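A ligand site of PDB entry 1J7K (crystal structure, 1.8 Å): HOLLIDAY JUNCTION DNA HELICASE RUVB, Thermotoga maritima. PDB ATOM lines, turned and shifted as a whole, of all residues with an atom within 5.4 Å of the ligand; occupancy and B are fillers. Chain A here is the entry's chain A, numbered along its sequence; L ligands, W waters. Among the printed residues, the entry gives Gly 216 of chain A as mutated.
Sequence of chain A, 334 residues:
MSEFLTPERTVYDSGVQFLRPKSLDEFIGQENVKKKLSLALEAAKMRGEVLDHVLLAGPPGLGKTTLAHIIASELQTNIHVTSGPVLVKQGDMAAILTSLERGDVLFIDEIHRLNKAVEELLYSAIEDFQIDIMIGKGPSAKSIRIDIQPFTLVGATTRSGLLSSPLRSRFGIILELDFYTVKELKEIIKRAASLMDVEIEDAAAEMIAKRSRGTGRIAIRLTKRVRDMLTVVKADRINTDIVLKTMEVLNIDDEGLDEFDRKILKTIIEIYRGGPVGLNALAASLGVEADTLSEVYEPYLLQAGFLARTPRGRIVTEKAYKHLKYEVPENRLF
An oxygen (O12) of the ligand sits at hydrogen-bond distance from the backbone carbonyl oxygen (O) of Gly 61, at 2.7 Å.
An oxygen (O2) of the ligand is in hydrogen-bond range of the backbone NH (N) of Gly 63.
O of Glu 26 lies within hydrogen-bond range of N3 of the ligand (3.0 Å).
The side-chain hydroxyl (OG1) of Thr 66 lies within hydrogen-bond range of an oxygen (O5) of the ligand (2.9 Å).
The backbone NH (N) of Leu 62 is in hydrogen-bond range of an oxygen (O2) of the ligand (3.3 Å).
The backbone carbonyl oxygen (O) of Leu 62 lies close to an oxygen (O12) of the ligand, at 3.4 Å.
An oxygen (O7) of the ligand is in salt-bridge range of the guanidinium group of Arg 20, 2.7 Å away.
An oxygen (O3) of the ligand is in hydrogen-bond range of the backbone NH of Thr 65 (2.8 Å).
The guanidinium group (NE) of Arg 217 is in salt-bridge range of an oxygen (O8) of the ligand.
The backbone NH (N) of Ile 28 is in hydrogen-bond range of a nitrogen (N2) of the ligand (2.8 Å).
The backbone NH of Gly 61 is in hydrogen-bond range of an oxygen (O1) of the ligand, at 2.8 Å.
The backbone NH of Lys 64 sits at hydrogen-bond distance from an oxygen (O2) of the ligand (2.8 Å).
The backbone NH (N) of Thr 66 lies within hydrogen-bond range of an oxygen (O5) of the ligand, 2.8 Å away.
An oxygen (O13) of the ligand sits at hydrogen-bond distance from the side-chain hydroxyl of Tyr 180 (3.3 Å).
An oxygen (O2) of the ligand is in salt-bridge range of the side-chain amino group (NZ) of Lys 64 (2.9 Å).
The side-chain hydroxyl (OG1) of Thr 65 sits at hydrogen-bond distance from an oxygen (O3) of the ligand (2.6 Å).
The backbone carbonyl oxygen of Gly 61 is in hydrogen-bond range of the backbone NH of Arg 217 (3.1 Å).
O of Leu 62 sits at hydrogen-bond distance from OH of Tyr 180 (2.7 Å).
OG1 of Thr 66 lies within hydrogen-bond range of NE of Arg 20 (3.2 Å).
NZ of Lys 64 sits at hydrogen-bond distance from O of Pro 59, at 2.9 Å.
The backbone carbonyl oxygen of Leu 19 sits close to a nitrogen (N4) of the ligand (3.3 Å).
Pro 21 touches the ligand.
Phe 27 touches the ligand.
Pro 60 touches the ligand (CA to O1, 3.6 Å).
Ile 188 touches the ligand (CD1 to O13, 3.0 Å).
Gly 216 touches the ligand (CA to O13, 3.2 Å).
CD1 of Ile 220 touches N5 of the ligand (3.6 Å).
18 residues have an atom within 4 Å of the ligand: Leu 19, Arg 20, Pro 21, Glu 26, Phe 27, Ile 28, Pro 60, Gly 61, Leu 62, Gly 63, Lys 64, Thr 65, Thr 66, Tyr 180, Ile 188, Gly 216, Arg 217 and Ile 220.
Along chain A the residues within 4 Å of the ligand span positions 19 to 220.
The nearest printed residue that does not touch the ligand is Pro 59 (4.1 Å).
Water W3 lies within hydrogen-bond range of O3 of the ligand (2.7 Å), OD1 of Asp 109 (2.9 Å) and OG1 of Thr 65 (3.5 Å).
Water W7 bridges a nitrogen (N4) of the ligand (2.7 Å) and the backbone carbonyl oxygen of Leu 19 (3.1 Å).
Water W6 lies within hydrogen-bond range of O4 of the ligand (2.8 Å), NH2 of Arg 217 (3.3 Å) and NH2 of Arg 20 (3.3 Å).
Water W5 bridges O1 of the ligand (2.9 Å) and NH2 of Arg 217 (3.1 Å).
Water W8 lies within hydrogen-bond range of the backbone carbonyl oxygen (O) of Glu 26 (3.0 Å), a nitrogen (N3) of the ligand (3.1 Å) and the guanidinium group (NE) of Arg 191 (3.3 Å).
Water W2 bridges NZ of Lys 64 (2.9 Å) and O1 of the ligand (3.4 Å).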
ATOM      1  N   LEU A  19      16.571 -14.461 -23.865  1.00  0.00           N
ATOM      2  CA  LEU A  19      17.751 -14.662 -22.974  1.00  0.00           C
ATOM      3  C   LEU A  19      17.527 -15.787 -21.958  1.00  0.00           C
ATOM      4  O   LEU A  19      18.399 -16.079 -21.140  1.00  0.00           O
ATOM      5  CB  LEU A  19      18.064 -13.361 -22.225  1.00  0.00           C
ATOM      6  CG  LEU A  19      18.610 -12.195 -23.061  1.00  0.00           C
ATOM      7  CD1 LEU A  19      18.647 -10.930 -22.227  1.00  0.00           C
ATOM      8  CD2 LEU A  19      20.002 -12.541 -23.576  1.00  0.00           C
ATOM      9  N   ARG A  20      16.362 -16.425 -22.031  1.00  0.00           N
ATOM     10  CA  ARG A  20      16.026 -17.522 -21.128  1.00  0.00           C
ATOM     11  C   ARG A  20      16.658 -18.838 -21.553  1.00  0.00           C
ATOM     12  O   ARG A  20      16.796 -19.110 -22.750  1.00  0.00           O
ATOM     13  CB  ARG A  20      14.511 -17.718 -21.057  1.00  0.00           C
ATOM     14  CG  ARG A  20      13.766 -16.727 -20.196  1.00  0.00           C
ATOM     15  CD  ARG A  20      12.276 -17.018 -20.224  1.00  0.00           C
ATOM     16  NE  ARG A  20      11.544 -16.173 -19.289  1.00  0.00           N
ATOM     17  CZ  ARG A  20      10.217 -16.099 -19.226  1.00  0.00           C
ATOM     18  NH1 ARG A  20       9.473 -16.820 -20.053  1.00  0.00           N
ATOM     19  NH2 ARG A  20       9.651 -15.311 -18.332  1.00  0.00           N
ATOM     20  N   PRO A  21      17.038 -19.685 -20.589  1.00  0.00           N
ATOM     21  CA  PRO A  21      17.641 -20.986 -20.892  1.00  0.00           C
ATOM     22  C   PRO A  21      16.578 -21.931 -21.436  1.00  0.00           C
ATOM     23  O   PRO A  21      15.386 -21.685 -21.274  1.00  0.00           O
ATOM     24  CB  PRO A  21      18.175 -21.433 -19.536  1.00  0.00           C
ATOM     25  CG  PRO A  21      17.177 -20.863 -18.585  1.00  0.00           C
ATOM     26  CD  PRO A  21      16.978 -19.461 -19.126  1.00  0.00           C
ATOM     27  N   GLU A  26      21.359 -25.633 -18.744  1.00  0.00           N
ATOM     28  CA  GLU A  26      21.680 -24.256 -19.105  1.00  0.00           C
ATOM     29  C   GLU A  26      21.248 -23.281 -18.013  1.00  0.00           C
ATOM     30  O   GLU A  26      21.549 -22.086 -18.096  1.00  0.00           O
ATOM     31  CB  GLU A  26      20.986 -23.886 -20.428  1.00  0.00           C
ATOM     32  CG  GLU A  26      21.472 -24.684 -21.627  1.00  0.00           C
ATOM     33  CD  GLU A  26      20.685 -24.398 -22.902  1.00  0.00           C
ATOM     34  OE1 GLU A  26      21.079 -24.926 -23.964  1.00  0.00           O
ATOM     35  OE2 GLU A  26      19.681 -23.653 -22.848  1.00  0.00           O
ATOM     36  N   PHE A  27      20.547 -23.790 -17.007  1.00  0.00           N
ATOM     37  CA  PHE A  27      20.057 -22.952 -15.898  1.00  0.00           C
ATOM     38  C   PHE A  27      21.092 -22.758 -14.801  1.00  0.00           C
ATOM     39  O   PHE A  27      21.552 -23.722 -14.178  1.00  0.00           O
ATOM     40  CB  PHE A  27      18.770 -23.561 -15.322  1.00  0.00           C
ATOM     41  CG  PHE A  27      17.963 -22.611 -14.463  1.00  0.00           C
ATOM     42  CD1 PHE A  27      18.381 -22.270 -13.175  1.00  0.00           C
ATOM     43  CD2 PHE A  27      16.787 -22.053 -14.950  1.00  0.00           C
ATOM     44  CE1 PHE A  27      17.623 -21.379 -12.387  1.00  0.00           C
ATOM     45  CE2 PHE A  27      16.029 -21.169 -14.174  1.00  0.00           C
ATOM     46  CZ  PHE A  27      16.451 -20.837 -12.889  1.00  0.00           C
ATOM     47  N   ILE A  28      21.465 -21.514 -14.570  1.00  0.00           N
ATOM     48  CA  ILE A  28      22.447 -21.155 -13.560  1.00  0.00           C
ATOM     49  C   ILE A  28      21.778 -20.916 -12.198  1.00  0.00           C
ATOM     50  O   ILE A  28      20.765 -20.221 -12.115  1.00  0.00           O
ATOM     51  CB  ILE A  28      23.212 -19.889 -13.983  1.00  0.00           C
ATOM     52  CG1 ILE A  28      23.959 -20.166 -15.284  1.00  0.00           C
ATOM     53  CG2 ILE A  28      24.132 -19.431 -12.870  1.00  0.00           C
ATOM     54  CD1 ILE A  28      24.311 -18.913 -16.075  1.00  0.00           C
ATOM     55  N   PRO A  59       9.980 -15.219  -4.641  1.00  0.00           N
ATOM     56  CA  PRO A  59       9.756 -13.862  -5.155  1.00  0.00           C
ATOM     57  C   PRO A  59       9.875 -13.749  -6.674  1.00  0.00           C
ATOM     58  O   PRO A  59      10.411 -14.627  -7.340  1.00  0.00           O
ATOM     59  CB  PRO A  59      10.805 -13.026  -4.403  1.00  0.00           C
ATOM     60  CG  PRO A  59      11.842 -14.021  -3.993  1.00  0.00           C
ATOM     61  CD  PRO A  59      11.056 -15.250  -3.643  1.00  0.00           C
ATOM     62  N   PRO A  60       9.351 -12.648  -7.243  1.00  0.00           N
ATOM     63  CA  PRO A  60       9.381 -12.406  -8.688  1.00  0.00           C
ATOM     64  C   PRO A  60      10.795 -12.315  -9.264  1.00  0.00           C
ATOM     65  O   PRO A  60      11.733 -11.918  -8.578  1.00  0.00           O
ATOM     66  CB  PRO A  60       8.622 -11.083  -8.830  1.00  0.00           C
ATOM     67  CG  PRO A  60       7.703 -11.078  -7.627  1.00  0.00           C
ATOM     68  CD  PRO A  60       8.605 -11.582  -6.545  1.00  0.00           C
ATOM     69  N   GLY A  61      10.936 -12.729 -10.524  1.00  0.00           N
ATOM     70  CA  GLY A  61      12.224 -12.651 -11.214  1.00  0.00           C
ATOM     71  C   GLY A  61      13.264 -13.698 -10.855  1.00  0.00           C
ATOM     72  O   GLY A  61      14.432 -13.550 -11.227  1.00  0.00           O
ATOM     73  N   LEU A  62      12.859 -14.757 -10.170  1.00  0.00           N
ATOM     74  CA  LEU A  62      13.799 -15.804  -9.782  1.00  0.00           C
ATOM     75  C   LEU A  62      13.879 -16.970 -10.747  1.00  0.00           C
ATOM     76  O   LEU A  62      14.715 -17.851 -10.600  1.00  0.00           O
ATOM     77  CB  LEU A  62      13.485 -16.323  -8.379  1.00  0.00           C
ATOM     78  CG  LEU A  62      13.754 -15.330  -7.250  1.00  0.00           C
ATOM     79  CD1 LEU A  62      13.431 -16.015  -5.919  1.00  0.00           C
ATOM     80  CD2 LEU A  62      15.201 -14.849  -7.267  1.00  0.00           C
ATOM     81  N   GLY A  63      13.011 -16.987 -11.748  1.00  0.00           N
ATOM     82  CA  GLY A  63      13.055 -18.061 -12.730  1.00  0.00           C
ATOM     83  C   GLY A  63      11.954 -19.111 -12.687  1.00  0.00           C
ATOM     84  O   GLY A  63      12.112 -20.171 -13.290  1.00  0.00           O
ATOM     85  N   LYS A  64      10.850 -18.831 -12.003  1.00  0.00           N
ATOM     86  CA  LYS A  64       9.752 -19.794 -11.939  1.00  0.00           C
ATOM     87  C   LYS A  64       9.159 -20.037 -13.328  1.00  0.00           C
ATOM     88  O   LYS A  64       8.998 -21.188 -13.740  1.00  0.00           O
ATOM     89  CB  LYS A  64       8.680 -19.282 -10.955  1.00  0.00           C
ATOM     90  CG  LYS A  64       9.214 -19.081  -9.526  1.00  0.00           C
ATOM     91  CD  LYS A  64       8.116 -18.688  -8.536  1.00  0.00           C
ATOM     92  CE  LYS A  64       7.488 -17.336  -8.857  1.00  0.00           C
ATOM     93  NZ  LYS A  64       8.462 -16.205  -8.730  1.00  0.00           N
ATOM     94  N   THR A  65       8.863 -18.951 -14.044  1.00  0.00           N
ATOM     95  CA  THR A  65       8.295 -19.047 -15.381  1.00  0.00           C
ATOM     96  C   THR A  65       9.296 -19.730 -16.305  1.00  0.00           C
ATOM     97  O   THR A  65       8.929 -20.563 -17.145  1.00  0.00           O
ATOM     98  CB  THR A  65       7.955 -17.639 -15.940  1.00  0.00           C
ATOM     99  OG1 THR A  65       6.994 -17.005 -15.093  1.00  0.00           O
ATOM    100  CG2 THR A  65       7.374 -17.746 -17.338  1.00  0.00           C
ATOM    101  N   THR A  66      10.560 -19.373 -16.145  1.00  0.00           N
ATOM    102  CA  THR A  66      11.629 -19.944 -16.951  1.00  0.00           C
ATOM    103  C   THR A  66      11.682 -21.461 -16.737  1.00  0.00           C
ATOM    104  O   THR A  66      11.762 -22.228 -17.715  1.00  0.00           O
ATOM    105  CB  THR A  66      12.973 -19.281 -16.578  1.00  0.00           C
ATOM    106  OG1 THR A  66      12.968 -17.923 -17.050  1.00  0.00           O
ATOM    107  CG2 THR A  66      14.140 -20.031 -17.186  1.00  0.00           C
ATOM    108  N   LEU A  67      11.624 -21.900 -15.480  1.00  0.00           N
ATOM    109  CA  LEU A  67      11.636 -23.317 -15.170  1.00  0.00           C
ATOM    110  C   LEU A  67      10.419 -24.045 -15.722  1.00  0.00           C
ATOM    111  O   LEU A  67      10.512 -25.191 -16.159  1.00  0.00           O
ATOM    112  CB  LEU A  67      11.738 -23.540 -13.656  1.00  0.00           C
ATOM    113  CG  LEU A  67      13.137 -23.242 -13.114  1.00  0.00           C
ATOM    114  CD1 LEU A  67      13.051 -23.018 -11.618  1.00  0.00           C
ATOM    115  CD2 LEU A  67      14.096 -24.391 -13.452  1.00  0.00           C
ATOM    116  N   ASP A 109       0.432 -19.131 -13.646  1.00  0.00           N
ATOM    117  CA  ASP A 109       1.182 -18.146 -12.874  1.00  0.00           C
ATOM    118  C   ASP A 109       0.187 -17.525 -11.896  1.00  0.00           C
ATOM    119  O   ASP A 109      -0.993 -17.411 -12.201  1.00  0.00           O
ATOM    120  CB  ASP A 109       1.773 -17.089 -13.808  1.00  0.00           C
ATOM    121  CG  ASP A 109       2.748 -16.178 -13.113  1.00  0.00           C
ATOM    122  OD1 ASP A 109       3.350 -16.605 -12.108  1.00  0.00           O
ATOM    123  OD2 ASP A 109       2.926 -15.023 -13.576  1.00  0.00           O
ATOM    124  N   LEU A 177      12.121 -21.483  -4.525  1.00  0.00           N
ATOM    125  CA  LEU A 177      13.270 -20.753  -5.041  1.00  0.00           C
ATOM    126  C   LEU A 177      13.748 -19.725  -4.025  1.00  0.00           C
ATOM    127  O   LEU A 177      12.949 -19.116  -3.321  1.00  0.00           O
ATOM    128  CB  LEU A 177      12.918 -20.042  -6.359  1.00  0.00           C
ATOM    129  CG  LEU A 177      12.830 -20.933  -7.601  1.00  0.00           C
ATOM    130  CD1 LEU A 177      11.637 -21.853  -7.494  1.00  0.00           C
ATOM    131  CD2 LEU A 177      12.737 -20.080  -8.863  1.00  0.00           C
ATOM    132  N   TYR A 180      19.449 -15.605  -5.409  1.00  0.00           N
ATOM    133  CA  TYR A 180      20.706 -16.118  -5.935  1.00  0.00           C
ATOM    134  C   TYR A 180      21.865 -15.529  -5.150  1.00  0.00           C
ATOM    135  O   TYR A 180      21.723 -14.459  -4.552  1.00  0.00           O
ATOM    136  CB  TYR A 180      20.912 -15.714  -7.397  1.00  0.00           C
ATOM    137  CG  TYR A 180      19.962 -16.357  -8.381  1.00  0.00           C
ATOM    138  CD1 TYR A 180      18.704 -15.814  -8.588  1.00  0.00           C
ATOM    139  CD2 TYR A 180      20.321 -17.505  -9.087  1.00  0.00           C
ATOM    140  CE1 TYR A 180      17.807 -16.392  -9.477  1.00  0.00           C
ATOM    141  CE2 TYR A 180      19.432 -18.101  -9.981  1.00  0.00           C
ATOM    142  CZ  TYR A 180      18.181 -17.538 -10.167  1.00  0.00           C
ATOM    143  OH  TYR A 180      17.329 -18.144 -11.044  1.00  0.00           O
ATOM    144  N   LEU A 185      24.796 -14.798  -9.612  1.00  0.00           N
ATOM    145  CA  LEU A 185      24.341 -13.628 -10.362  1.00  0.00           C
ATOM    146  C   LEU A 185      25.433 -13.185 -11.327  1.00  0.00           C
ATOM    147  O   LEU A 185      25.155 -12.854 -12.475  1.00  0.00           O
ATOM    148  CB  LEU A 185      23.979 -12.495  -9.397  1.00  0.00           C
ATOM    149  CG  LEU A 185      22.702 -12.770  -8.586  1.00  0.00           C
ATOM    150  CD1 LEU A 185      22.476 -11.679  -7.539  1.00  0.00           C
ATOM    151  CD2 LEU A 185      21.513 -12.846  -9.530  1.00  0.00           C
ATOM    152  N   ILE A 188      25.367 -15.261 -14.306  1.00  0.00           N
ATOM    153  CA  ILE A 188      24.218 -14.915 -15.136  1.00  0.00           C
ATOM    154  C   ILE A 188      24.505 -13.634 -15.929  1.00  0.00           C
ATOM    155  O   ILE A 188      24.177 -13.545 -17.121  1.00  0.00           O
ATOM    156  CB  ILE A 188      22.958 -14.730 -14.249  1.00  0.00           C
ATOM    157  CG1 ILE A 188      22.560 -16.086 -13.638  1.00  0.00           C
ATOM    158  CG2 ILE A 188      21.812 -14.155 -15.061  1.00  0.00           C
ATOM    159  CD1 ILE A 188      21.611 -16.005 -12.466  1.00  0.00           C
ATOM    160  N   ARG A 191      26.910 -14.313 -18.705  1.00  0.00           N
ATOM    161  CA  ARG A 191      26.213 -15.038 -19.769  1.00  0.00           C
ATOM    162  C   ARG A 191      25.379 -14.069 -20.610  1.00  0.00           C
ATOM    163  O   ARG A 191      25.383 -14.132 -21.835  1.00  0.00           O
ATOM    164  CB  ARG A 191      25.322 -16.120 -19.174  1.00  0.00           C
ATOM    165  CG  ARG A 191      24.526 -16.904 -20.205  1.00  0.00           C
ATOM    166  CD  ARG A 191      25.431 -17.735 -21.099  1.00  0.00           C
ATOM    167  NE  ARG A 191      24.662 -18.670 -21.912  1.00  0.00           N
ATOM    168  CZ  ARG A 191      25.186 -19.699 -22.559  1.00  0.00           C
ATOM    169  NH1 ARG A 191      24.409 -20.506 -23.276  1.00  0.00           N
ATOM    170  NH2 ARG A 191      26.490 -19.944 -22.484  1.00  0.00           N
ATOM    171  N   THR A 215      18.240 -11.102  -7.299  1.00  0.00           N
ATOM    172  CA  THR A 215      17.342 -11.508  -8.360  1.00  0.00           C
ATOM    173  C   THR A 215      17.899 -11.572  -9.784  1.00  0.00           C
ATOM    174  O   THR A 215      18.366 -10.570 -10.307  1.00  0.00           O
ATOM    175  CB  THR A 215      16.147 -10.574  -8.324  1.00  0.00           C
ATOM    176  OG1 THR A 215      15.659 -10.522  -6.972  1.00  0.00           O
ATOM    177  CG2 THR A 215      15.051 -11.040  -9.248  1.00  0.00           C
ATOM    178  N   GLY A 216      17.812 -12.743 -10.413  1.00  0.00           N
ATOM    179  CA  GLY A 216      18.300 -12.898 -11.767  1.00  0.00           C
ATOM    180  C   GLY A 216      17.738 -11.907 -12.769  1.00  0.00           C
ATOM    181  O   GLY A 216      18.472 -11.343 -13.575  1.00  0.00           O
ATOM    182  N   ARG A 217      16.426 -11.704 -12.760  1.00  0.00           N
ATOM    183  CA  ARG A 217      15.820 -10.767 -13.698  1.00  0.00           C
ATOM    184  C   ARG A 217      16.451  -9.378 -13.562  1.00  0.00           C
ATOM    185  O   ARG A 217      16.756  -8.728 -14.565  1.00  0.00           O
ATOM    186  CB  ARG A 217      14.311 -10.707 -13.476  1.00  0.00           C
ATOM    187  CG  ARG A 217      13.640  -9.575 -14.221  1.00  0.00           C
ATOM    188  CD  ARG A 217      12.185  -9.488 -13.856  1.00  0.00           C
ATOM    189  NE  ARG A 217      11.438 -10.655 -14.317  1.00  0.00           N
ATOM    190  CZ  ARG A 217      10.215 -10.956 -13.910  1.00  0.00           C
ATOM    191  NH1 ARG A 217       9.608 -10.177 -13.012  1.00  0.00           N
ATOM    192  NH2 ARG A 217       9.595 -12.035 -14.378  1.00  0.00           N
ATOM    193  N   ILE A 220      20.026  -9.240 -15.061  1.00  0.00           N
ATOM    194  CA  ILE A 220      19.995  -9.186 -16.517  1.00  0.00           C
ATOM    195  C   ILE A 220      19.592  -7.790 -17.031  1.00  0.00           C
ATOM    196  O   ILE A 220      20.219  -7.253 -17.949  1.00  0.00           O
ATOM    197  CB  ILE A 220      19.032 -10.250 -17.084  1.00  0.00           C
ATOM    198  CG1 ILE A 220      19.570 -11.640 -16.743  1.00  0.00           C
ATOM    199  CG2 ILE A 220      18.873 -10.075 -18.604  1.00  0.00           C
ATOM    200  CD1 ILE A 220      18.559 -12.760 -16.887  1.00  0.00           C
HETATM  201  P1  LIG L   1       9.557 -15.568 -12.209  1.00  0.00           P
HETATM  202  O1  LIG L   1       9.031 -14.292 -11.789  1.00  0.00           O
HETATM  203  O2  LIG L   1      10.147 -16.325 -11.101  1.00  0.00           O
HETATM  204  O3  LIG L   1       8.515 -16.324 -13.052  1.00  0.00           O
HETATM  205  P2  LIG L   1      11.065 -15.426 -14.758  1.00  0.00           P
HETATM  206  O4  LIG L   1      10.046 -14.625 -15.504  1.00  0.00           O
HETATM  207  O5  LIG L   1      11.193 -16.864 -15.062  1.00  0.00           O
HETATM  208  O6  LIG L   1      10.791 -15.175 -13.162  1.00  0.00           O
HETATM  209  P3  LIG L   1      13.056 -13.891 -16.124  1.00  0.00           P
HETATM  210  O7  LIG L   1      12.720 -14.664 -17.317  1.00  0.00           O
HETATM  211  O8  LIG L   1      12.714 -12.445 -16.091  1.00  0.00           O
HETATM  212  O9  LIG L   1      12.408 -14.691 -14.928  1.00  0.00           O
HETATM  213  O10 LIG L   1      14.588 -14.066 -15.849  1.00  0.00           O
HETATM  214  C1  LIG L   1      15.273 -15.318 -16.069  1.00  0.00           C
HETATM  215  C2  LIG L   1      15.543 -15.967 -14.743  1.00  0.00           C
HETATM  216  O11 LIG L   1      16.199 -17.224 -15.061  1.00  0.00           O
HETATM  217  C3  LIG L   1      16.480 -15.180 -13.832  1.00  0.00           C
HETATM  218  O12 LIG L   1      15.980 -15.317 -12.489  1.00  0.00           O
HETATM  219  C4  LIG L   1      17.781 -15.871 -14.063  1.00  0.00           C
HETATM  220  O13 LIG L   1      18.673 -15.818 -12.960  1.00  0.00           O
HETATM  221  C5  LIG L   1      17.443 -17.325 -14.346  1.00  0.00           C
HETATM  222  N1  LIG L   1      18.469 -17.993 -15.169  1.00  0.00           N
HETATM  223  C6  LIG L   1      19.105 -19.176 -14.927  1.00  0.00           C
HETATM  224  N2  LIG L   1      19.977 -19.540 -15.811  1.00  0.00           N
HETATM  225  C7  LIG L   1      19.918 -18.501 -16.737  1.00  0.00           C
HETATM  226  C8  LIG L   1      20.616 -18.263 -17.951  1.00  0.00           C
HETATM  227  N3  LIG L   1      21.531 -19.109 -18.395  1.00  0.00           N
HETATM  228  N4  LIG L   1      20.340 -17.124 -18.657  1.00  0.00           N
HETATM  229  C9  LIG L   1      19.420 -16.276 -18.189  1.00  0.00           C
HETATM  230  N5  LIG L   1      18.688 -16.378 -17.053  1.00  0.00           N
HETATM  231  C10 LIG L   1      18.990 -17.547 -16.361  1.00  0.00           C
HETATM  232  O   HOH W   1      14.765 -11.037 -17.618  1.00  0.00           O
HETATM  233  O   HOH W   2       6.433 -14.250  -9.551  1.00  0.00           O
HETATM  234  O   HOH W   3       6.176 -16.313 -11.790  1.00  0.00           O
HETATM  235  O   HOH W   4      20.052 -18.140 -21.984  1.00  0.00           O
HETATM  236  O   HOH W   5       6.895 -12.750 -13.066  1.00  0.00           O
HETATM  237  O   HOH W   6       7.558 -13.729 -16.291  1.00  0.00           O
HETATM  238  O   HOH W   7      21.512 -16.286 -20.926  1.00  0.00           O
HETATM  239  O   HOH W   8      23.788 -20.867 -19.614  1.00  0.00           O
